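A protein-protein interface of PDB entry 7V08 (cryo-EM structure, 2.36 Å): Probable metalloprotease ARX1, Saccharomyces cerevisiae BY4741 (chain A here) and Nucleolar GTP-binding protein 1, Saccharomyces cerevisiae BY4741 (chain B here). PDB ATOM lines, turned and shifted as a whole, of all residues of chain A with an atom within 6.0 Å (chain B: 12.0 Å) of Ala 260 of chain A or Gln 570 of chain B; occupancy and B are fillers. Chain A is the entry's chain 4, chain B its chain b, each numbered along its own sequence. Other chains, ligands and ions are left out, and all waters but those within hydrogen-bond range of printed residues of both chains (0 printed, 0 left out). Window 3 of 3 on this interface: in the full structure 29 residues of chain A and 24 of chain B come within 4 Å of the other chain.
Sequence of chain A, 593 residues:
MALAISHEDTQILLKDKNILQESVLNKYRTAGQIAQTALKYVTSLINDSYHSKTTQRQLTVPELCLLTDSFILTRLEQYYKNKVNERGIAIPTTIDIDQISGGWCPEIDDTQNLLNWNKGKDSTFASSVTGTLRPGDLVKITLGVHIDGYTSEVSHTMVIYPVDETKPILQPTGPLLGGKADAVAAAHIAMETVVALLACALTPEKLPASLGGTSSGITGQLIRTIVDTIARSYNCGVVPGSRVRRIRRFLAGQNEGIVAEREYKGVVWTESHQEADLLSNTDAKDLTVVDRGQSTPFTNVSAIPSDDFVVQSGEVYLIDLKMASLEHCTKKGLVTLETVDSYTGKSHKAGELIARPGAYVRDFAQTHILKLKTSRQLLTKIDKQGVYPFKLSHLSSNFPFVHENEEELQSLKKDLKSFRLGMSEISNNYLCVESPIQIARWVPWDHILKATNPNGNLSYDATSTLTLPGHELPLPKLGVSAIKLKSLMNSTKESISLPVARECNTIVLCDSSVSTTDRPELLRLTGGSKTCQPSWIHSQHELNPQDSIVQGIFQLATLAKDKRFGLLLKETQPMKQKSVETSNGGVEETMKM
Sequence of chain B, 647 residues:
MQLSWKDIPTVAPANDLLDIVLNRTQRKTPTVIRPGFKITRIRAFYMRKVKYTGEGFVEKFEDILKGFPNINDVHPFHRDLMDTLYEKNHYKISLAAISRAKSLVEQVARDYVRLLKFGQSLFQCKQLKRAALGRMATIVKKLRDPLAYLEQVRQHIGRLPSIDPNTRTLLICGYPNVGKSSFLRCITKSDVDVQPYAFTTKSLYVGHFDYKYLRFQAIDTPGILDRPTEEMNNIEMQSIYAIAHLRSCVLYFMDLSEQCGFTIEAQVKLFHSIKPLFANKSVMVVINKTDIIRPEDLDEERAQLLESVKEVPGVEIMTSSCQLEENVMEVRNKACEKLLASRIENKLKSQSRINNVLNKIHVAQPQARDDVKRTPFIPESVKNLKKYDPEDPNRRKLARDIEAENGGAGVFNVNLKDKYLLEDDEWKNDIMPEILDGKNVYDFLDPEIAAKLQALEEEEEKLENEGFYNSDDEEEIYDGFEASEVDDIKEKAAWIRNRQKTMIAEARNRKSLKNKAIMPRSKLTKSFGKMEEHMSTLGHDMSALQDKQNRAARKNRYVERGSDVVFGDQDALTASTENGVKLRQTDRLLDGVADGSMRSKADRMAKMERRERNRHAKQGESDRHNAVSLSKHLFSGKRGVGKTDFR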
ATOM      1  N   ASN A 255      32.241   4.067 -14.371  1.00  0.00           N
ATOM      2  CA  ASN A 255      31.857   2.654 -14.350  1.00  0.00           C
ATOM      3  C   ASN A 255      30.338   2.603 -14.486  1.00  0.00           C
ATOM      4  O   ASN A 255      29.616   2.530 -13.491  1.00  0.00           O
ATOM      5  CB  ASN A 255      32.343   1.965 -13.084  1.00  0.00           C
ATOM      6  CG  ASN A 255      32.587   2.940 -11.952  1.00  0.00           C
ATOM      7  OD1 ASN A 255      31.764   3.817 -11.685  1.00  0.00           O
ATOM      8  ND2 ASN A 255      33.728   2.801 -11.289  1.00  0.00           N
ATOM      9  N   GLU A 256      29.863   2.615 -15.732  1.00  0.00           N
ATOM     10  CA  GLU A 256      28.430   2.724 -15.980  1.00  0.00           C
ATOM     11  C   GLU A 256      27.744   1.365 -15.900  1.00  0.00           C
ATOM     12  O   GLU A 256      26.633   1.254 -15.373  1.00  0.00           O
ATOM     13  CB  GLU A 256      28.192   3.387 -17.338  1.00  0.00           C
ATOM     14  CG  GLU A 256      26.729   3.561 -17.697  1.00  0.00           C
ATOM     15  CD  GLU A 256      26.454   4.878 -18.390  1.00  0.00           C
ATOM     16  OE1 GLU A 256      27.266   5.809 -18.236  1.00  0.00           O
ATOM     17  OE2 GLU A 256      25.424   4.986 -19.085  1.00  0.00           O
ATOM     18  N   ILE A 258      28.563  -1.046 -13.997  1.00  0.00           N
ATOM     19  CA  ILE A 258      28.862  -1.660 -12.705  1.00  0.00           C
ATOM     20  C   ILE A 258      28.194  -0.900 -11.558  1.00  0.00           C
ATOM     21  O   ILE A 258      27.491  -1.493 -10.737  1.00  0.00           O
ATOM     22  CB  ILE A 258      30.387  -1.774 -12.490  1.00  0.00           C
ATOM     23  CG1 ILE A 258      31.036  -2.477 -13.683  1.00  0.00           C
ATOM     24  CG2 ILE A 258      30.692  -2.525 -11.209  1.00  0.00           C
ATOM     25  CD1 ILE A 258      32.497  -2.165 -13.848  1.00  0.00           C
ATOM     26  N   VAL A 259      28.400   0.412 -11.485  1.00  0.00           N
ATOM     27  CA  VAL A 259      27.868   1.241 -10.407  1.00  0.00           C
ATOM     28  C   VAL A 259      26.583   1.907 -10.882  1.00  0.00           C
ATOM     29  O   VAL A 259      26.505   2.375 -12.025  1.00  0.00           O
ATOM     30  CB  VAL A 259      28.897   2.287  -9.945  1.00  0.00           C
ATOM     31  CG1 VAL A 259      28.360   3.088  -8.767  1.00  0.00           C
ATOM     32  CG2 VAL A 259      30.205   1.618  -9.569  1.00  0.00           C
ATOM     33  N   ALA A 260      25.568   1.924 -10.018  1.00  0.00           N
ATOM     34  CA  ALA A 260      24.292   2.557 -10.325  1.00  0.00           C
ATOM     35  C   ALA A 260      24.302   4.035  -9.947  1.00  0.00           C
ATOM     36  O   ALA A 260      25.084   4.478  -9.100  1.00  0.00           O
ATOM     37  CB  ALA A 260      23.153   1.851  -9.590  1.00  0.00           C
ATOM     38  N   GLU A 261      23.412   4.797 -10.581  1.00  0.00           N
ATOM     39  CA  GLU A 261      23.311   6.234 -10.374  1.00  0.00           C
ATOM     40  C   GLU A 261      21.866   6.620 -10.089  1.00  0.00           C
ATOM     41  O   GLU A 261      20.931   6.050 -10.654  1.00  0.00           O
ATOM     42  CB  GLU A 261      23.820   7.015 -11.591  1.00  0.00           C
ATOM     43  CG  GLU A 261      25.265   6.722 -11.952  1.00  0.00           C
ATOM     44  CD  GLU A 261      25.664   7.315 -13.287  1.00  0.00           C
ATOM     45  OE1 GLU A 261      25.091   8.356 -13.675  1.00  0.00           O
ATOM     46  OE2 GLU A 261      26.547   6.735 -13.949  1.00  0.00           O
ATOM     47  N   ARG A 262      21.700   7.607  -9.206  1.00  0.00           N
ATOM     48  CA  ARG A 262      20.366   8.066  -8.831  1.00  0.00           C
ATOM     49  C   ARG A 262      19.692   8.813  -9.973  1.00  0.00           C
ATOM     50  O   ARG A 262      18.533   8.538 -10.309  1.00  0.00           O
ATOM     51  CB  ARG A 262      20.448   8.952  -7.590  1.00  0.00           C
ATOM     52  CG  ARG A 262      20.600   8.184  -6.294  1.00  0.00           C
ATOM     53  CD  ARG A 262      19.384   7.308  -6.052  1.00  0.00           C
ATOM     54  NE  ARG A 262      19.329   6.791  -4.689  1.00  0.00           N
ATOM     55  CZ  ARG A 262      19.619   5.544  -4.345  1.00  0.00           C
ATOM     56  NH1 ARG A 262      19.999   4.650  -5.242  1.00  0.00           N
ATOM     57  NH2 ARG A 262      19.521   5.186  -3.069  1.00  0.00           N
ATOM     58  N   ALA A 365      30.408   0.695  -0.553  1.00  0.00           N
ATOM     59  CA  ALA A 365      29.300   0.324   0.317  1.00  0.00           C
ATOM     60  C   ALA A 365      29.522  -1.009   1.018  1.00  0.00           C
ATOM     61  O   ALA A 365      28.717  -1.381   1.876  1.00  0.00           O
ATOM     62  CB  ALA A 365      27.995   0.279  -0.482  1.00  0.00           C
ATOM     63  N   LEU A 468      23.744  -5.541 -11.588  1.00  0.00           N
ATOM     64  CA  LEU A 468      23.231  -4.734 -12.697  1.00  0.00           C
ATOM     65  C   LEU A 468      23.151  -5.491 -14.023  1.00  0.00           C
ATOM     66  O   LEU A 468      22.083  -5.451 -14.658  1.00  0.00           O
ATOM     67  CB  LEU A 468      24.055  -3.445 -12.825  1.00  0.00           C
ATOM     68  CG  LEU A 468      23.379  -2.144 -12.385  1.00  0.00           C
ATOM     69  CD1 LEU A 468      23.094  -2.160 -10.891  1.00  0.00           C
ATOM     70  CD2 LEU A 468      24.219  -0.930 -12.772  1.00  0.00           C
ATOM     71  N   ARG B 561      33.752  13.431   0.424  1.00  0.00           N
ATOM     72  CA  ARG B 561      34.628  12.916  -0.614  1.00  0.00           C
ATOM     73  C   ARG B 561      33.799  12.242  -1.701  1.00  0.00           C
ATOM     74  O   ARG B 561      32.562  12.168  -1.633  1.00  0.00           O
ATOM     75  CB  ARG B 561      35.663  11.947  -0.027  1.00  0.00           C
ATOM     76  CG  ARG B 561      36.707  12.627   0.835  1.00  0.00           C
ATOM     77  CD  ARG B 561      37.792  11.659   1.267  1.00  0.00           C
ATOM     78  NE  ARG B 561      37.259  10.548   2.046  1.00  0.00           N
ATOM     79  CZ  ARG B 561      36.992  10.601   3.342  1.00  0.00           C
ATOM     80  NH1 ARG B 561      37.163  11.712   4.040  1.00  0.00           N
ATOM     81  NH2 ARG B 561      36.536   9.512   3.957  1.00  0.00           N
ATOM     82  N   GLY B 562      34.508  11.747  -2.719  1.00  0.00           N
ATOM     83  CA  GLY B 562      33.842  11.113  -3.844  1.00  0.00           C
ATOM     84  C   GLY B 562      33.068   9.872  -3.449  1.00  0.00           C
ATOM     85  O   GLY B 562      32.000   9.601  -4.000  1.00  0.00           O
ATOM     86  N   SER B 563      33.596   9.101  -2.494  1.00  0.00           N
ATOM     87  CA  SER B 563      32.868   7.937  -1.994  1.00  0.00           C
ATOM     88  C   SER B 563      31.572   8.354  -1.311  1.00  0.00           C
ATOM     89  O   SER B 563      30.545   7.681  -1.453  1.00  0.00           O
ATOM     90  CB  SER B 563      33.748   7.124  -1.045  1.00  0.00           C
ATOM     91  OG  SER B 563      34.100   7.876   0.099  1.00  0.00           O
ATOM     92  N   ASP B 564      31.598   9.464  -0.571  1.00  0.00           N
ATOM     93  CA  ASP B 564      30.370   9.998   0.008  1.00  0.00           C
ATOM     94  C   ASP B 564      29.377  10.432  -1.063  1.00  0.00           C
ATOM     95  O   ASP B 564      28.166  10.262  -0.884  1.00  0.00           O
ATOM     96  CB  ASP B 564      30.690  11.171   0.934  1.00  0.00           C
ATOM     97  CG  ASP B 564      31.490  10.752   2.150  1.00  0.00           C
ATOM     98  OD1 ASP B 564      31.200   9.679   2.711  1.00  0.00           O
ATOM     99  OD2 ASP B 564      32.415  11.492   2.542  1.00  0.00           O
ATOM    100  N   VAL B 565      29.857  11.007  -2.170  1.00  0.00           N
ATOM    101  CA  VAL B 565      28.942  11.416  -3.237  1.00  0.00           C
ATOM    102  C   VAL B 565      28.343  10.199  -3.941  1.00  0.00           C
ATOM    103  O   VAL B 565      27.139  10.154  -4.215  1.00  0.00           O
ATOM    104  CB  VAL B 565      29.656  12.349  -4.235  1.00  0.00           C
ATOM    105  CG1 VAL B 565      28.776  12.618  -5.443  1.00  0.00           C
ATOM    106  CG2 VAL B 565      30.030  13.660  -3.571  1.00  0.00           C
ATOM    107  N   VAL B 566      29.163   9.198  -4.242  1.00  0.00           N
ATOM    108  CA  VAL B 566      28.736   8.101  -5.108  1.00  0.00           C
ATOM    109  C   VAL B 566      28.025   7.004  -4.329  1.00  0.00           C
ATOM    110  O   VAL B 566      26.905   6.620  -4.669  1.00  0.00           O
ATOM    111  CB  VAL B 566      29.943   7.541  -5.892  1.00  0.00           C
ATOM    112  CG1 VAL B 566      29.510   6.371  -6.760  1.00  0.00           C
ATOM    113  CG2 VAL B 566      30.551   8.626  -6.739  1.00  0.00           C
ATOM    114  N   PHE B 567      28.652   6.473  -3.279  1.00  0.00           N
ATOM    115  CA  PHE B 567      28.177   5.266  -2.614  1.00  0.00           C
ATOM    116  C   PHE B 567      27.411   5.560  -1.328  1.00  0.00           C
ATOM    117  O   PHE B 567      27.021   4.632  -0.615  1.00  0.00           O
ATOM    118  CB  PHE B 567      29.348   4.329  -2.324  1.00  0.00           C
ATOM    119  CG  PHE B 567      30.071   3.867  -3.551  1.00  0.00           C
ATOM    120  CD1 PHE B 567      29.667   2.726  -4.222  1.00  0.00           C
ATOM    121  CD2 PHE B 567      31.154   4.573  -4.037  1.00  0.00           C
ATOM    122  CE1 PHE B 567      30.331   2.302  -5.349  1.00  0.00           C
ATOM    123  CE2 PHE B 567      31.820   4.154  -5.157  1.00  0.00           C
ATOM    124  CZ  PHE B 567      31.405   3.021  -5.821  1.00  0.00           C
ATOM    125  N   GLY B 568      27.171   6.837  -1.029  1.00  0.00           N
ATOM    126  CA  GLY B 568      26.605   7.193   0.264  1.00  0.00           C
ATOM    127  C   GLY B 568      25.205   6.647   0.492  1.00  0.00           C
ATOM    128  O   GLY B 568      24.908   6.112   1.562  1.00  0.00           O
ATOM    129  N   ASP B 569      24.331   6.763  -0.506  1.00  0.00           N
ATOM    130  CA  ASP B 569      22.968   6.269  -0.381  1.00  0.00           C
ATOM    131  C   ASP B 569      22.738   4.938  -1.082  1.00  0.00           C
ATOM    132  O   ASP B 569      21.642   4.377  -0.965  1.00  0.00           O
ATOM    133  CB  ASP B 569      21.975   7.300  -0.929  1.00  0.00           C
ATOM    134  CG  ASP B 569      22.252   7.661  -2.366  1.00  0.00           C
ATOM    135  OD1 ASP B 569      23.442   7.703  -2.747  1.00  0.00           O
ATOM    136  OD2 ASP B 569      21.281   7.896  -3.114  1.00  0.00           O
ATOM    137  N   GLN B 570      23.726   4.425  -1.804  1.00  0.00           N
ATOM    138  CA  GLN B 570      23.593   3.143  -2.470  1.00  0.00           C
ATOM    139  C   GLN B 570      23.994   2.007  -1.532  1.00  0.00           C
ATOM    140  O   GLN B 570      24.335   2.212  -0.364  1.00  0.00           O
ATOM    141  CB  GLN B 570      24.437   3.117  -3.740  1.00  0.00           C
ATOM    142  CG  GLN B 570      24.062   4.187  -4.741  1.00  0.00           C
ATOM    143  CD  GLN B 570      25.046   4.277  -5.885  1.00  0.00           C
ATOM    144  OE1 GLN B 570      25.995   3.502  -5.965  1.00  0.00           O
ATOM    145  NE2 GLN B 570      24.824   5.234  -6.782  1.00  0.00           N
ATOM    146  N   ASP B 571      23.935   0.788  -2.060  1.00  0.00           N
ATOM    147  CA  ASP B 571      24.360  -0.393  -1.326  1.00  0.00           C
ATOM    148  C   ASP B 571      24.739  -1.470  -2.331  1.00  0.00           C
ATOM    149  O   ASP B 571      24.918  -1.201  -3.522  1.00  0.00           O
ATOM    150  CB  ASP B 571      23.265  -0.882  -0.374  1.00  0.00           C
ATOM    151  CG  ASP B 571      23.716  -2.056   0.475  1.00  0.00           C
ATOM    152  OD1 ASP B 571      24.883  -2.476   0.337  1.00  0.00           O
ATOM    153  OD2 ASP B 571      22.913  -2.550   1.296  1.00  0.00           O
ATOM    154  N   ALA B 572      24.896  -2.689  -1.820  1.00  0.00           N
ATOM    155  CA  ALA B 572      25.038  -3.896  -2.625  1.00  0.00           C
ATOM    156  C   ALA B 572      26.226  -3.836  -3.572  1.00  0.00           C
ATOM    157  O   ALA B 572      27.369  -4.031  -3.152  1.00  0.00           O
ATOM    158  CB  ALA B 572      23.752  -4.161  -3.416  1.00  0.00           C
ATOM    159  N   LEU B 573      25.955  -3.557  -4.848  1.00  0.00           N
ATOM    160  CA  LEU B 573      26.873  -3.657  -5.980  1.00  0.00           C
ATOM    161  C   LEU B 573      27.393  -5.076  -6.180  1.00  0.00           C
ATOM    162  O   LEU B 573      28.365  -5.266  -6.916  1.00  0.00           O
ATOM    163  CB  LEU B 573      28.069  -2.702  -5.869  1.00  0.00           C
ATOM    164  CG  LEU B 573      29.105  -2.806  -6.985  1.00  0.00           C
ATOM    165  CD1 LEU B 573      28.462  -2.434  -8.313  1.00  0.00           C
ATOM    166  CD2 LEU B 573      30.311  -1.932  -6.691  1.00  0.00           C
ATOM    167  N   THR B 574      26.794  -6.072  -5.537  1.00  0.00           N
ATOM    168  CA  THR B 574      27.149  -7.470  -5.733  1.00  0.00           C
ATOM    169  C   THR B 574      25.924  -8.291  -5.367  1.00  0.00           C
ATOM    170  O   THR B 574      25.237  -7.972  -4.390  1.00  0.00           O
ATOM    171  CB  THR B 574      28.380  -7.856  -4.893  1.00  0.00           C
ATOM    172  OG1 THR B 574      29.499  -7.057  -5.298  1.00  0.00           O
ATOM    173  CG2 THR B 574      28.732  -9.331  -5.029  1.00  0.00           C
ATOM    174  N   ALA B 575      25.617  -9.296  -6.186  1.00  0.00           N
ATOM    175  CA  ALA B 575      24.454 -10.140  -5.944  1.00  0.00           C
ATOM    176  C   ALA B 575      24.611 -10.892  -4.631  1.00  0.00           C
ATOM    177  O   ALA B 575      25.617 -11.571  -4.413  1.00  0.00           O
ATOM    178  CB  ALA B 575      24.266 -11.119  -7.101  1.00  0.00           C
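Printed residues of chain B that touch a printed residue of chain A: Asp 569, Gln 570, Asp 571 and Leu 573. Of the 9 printed residues of chain A, 5 touch a printed residue of chain B. Hydrophobic or aromatic side chains of chain A that line the printed part of chain B: Ile 258, Val 259 and Ala 365.
Leu 573 of chain B touches Ile 258 of chain A (CD1 to O, 2.8 Å). CG1 of Val 259 of chain A touches OE1 of Gln 570 of chain B, 3.7 Å away. CB of Ala 365 of chain A touches CA of Asp 571 of chain B (3.8 Å).
The guanidinium group (NE) of Arg 262 of chain A is in salt-bridge range of the side-chain carboxylate (OD2) of Asp 569 of chain B, 2.7 Å away. The backbone carbonyl oxygen (O) of Ala 260 of chain A lies within hydrogen-bond range of the side-chain amide nitrogen (NE2) of Gln 570 of chain B.
Of chain B, only Gln 570 comes within 4 Å of Ala 260 of chain A. Of chain A, only Val 259 (3.7 Å) and Ala 260 (2.5 Å) come within 4 Å of Gln 570 of chain B. Printed residues of chain B within 4 Å of Arg 262 of chain A: Asp 569 (2.7 Å). Ala 365 of chain A touches just one residue of chain B: Asp 571 (3.8 Å). Of the printed residues of chain B, Ile 258 of chain A touches Leu 573. Of the printed residues of chain A, Asp 569 of chain B touches Arg 262. Printed residues of chain B within 4 Å of Val 259 of chain A: Gln 570 (3.7 Å). Printed residues of chain A within 4 Å of Leu 573 of chain B: Ile 258 (2.8 Å). The nearest residue of chain A that does not touch Gln 570 of chain B is Glu 261 of chain A (4.02 Å). The nearest printed residue of chain A that does not touch Asp 569 of chain B is Ala 365 of chain A (7.0 Å).
NE2 of Gln 570 of chain B lies close to O of Val 566 of chain B (3.3 Å).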
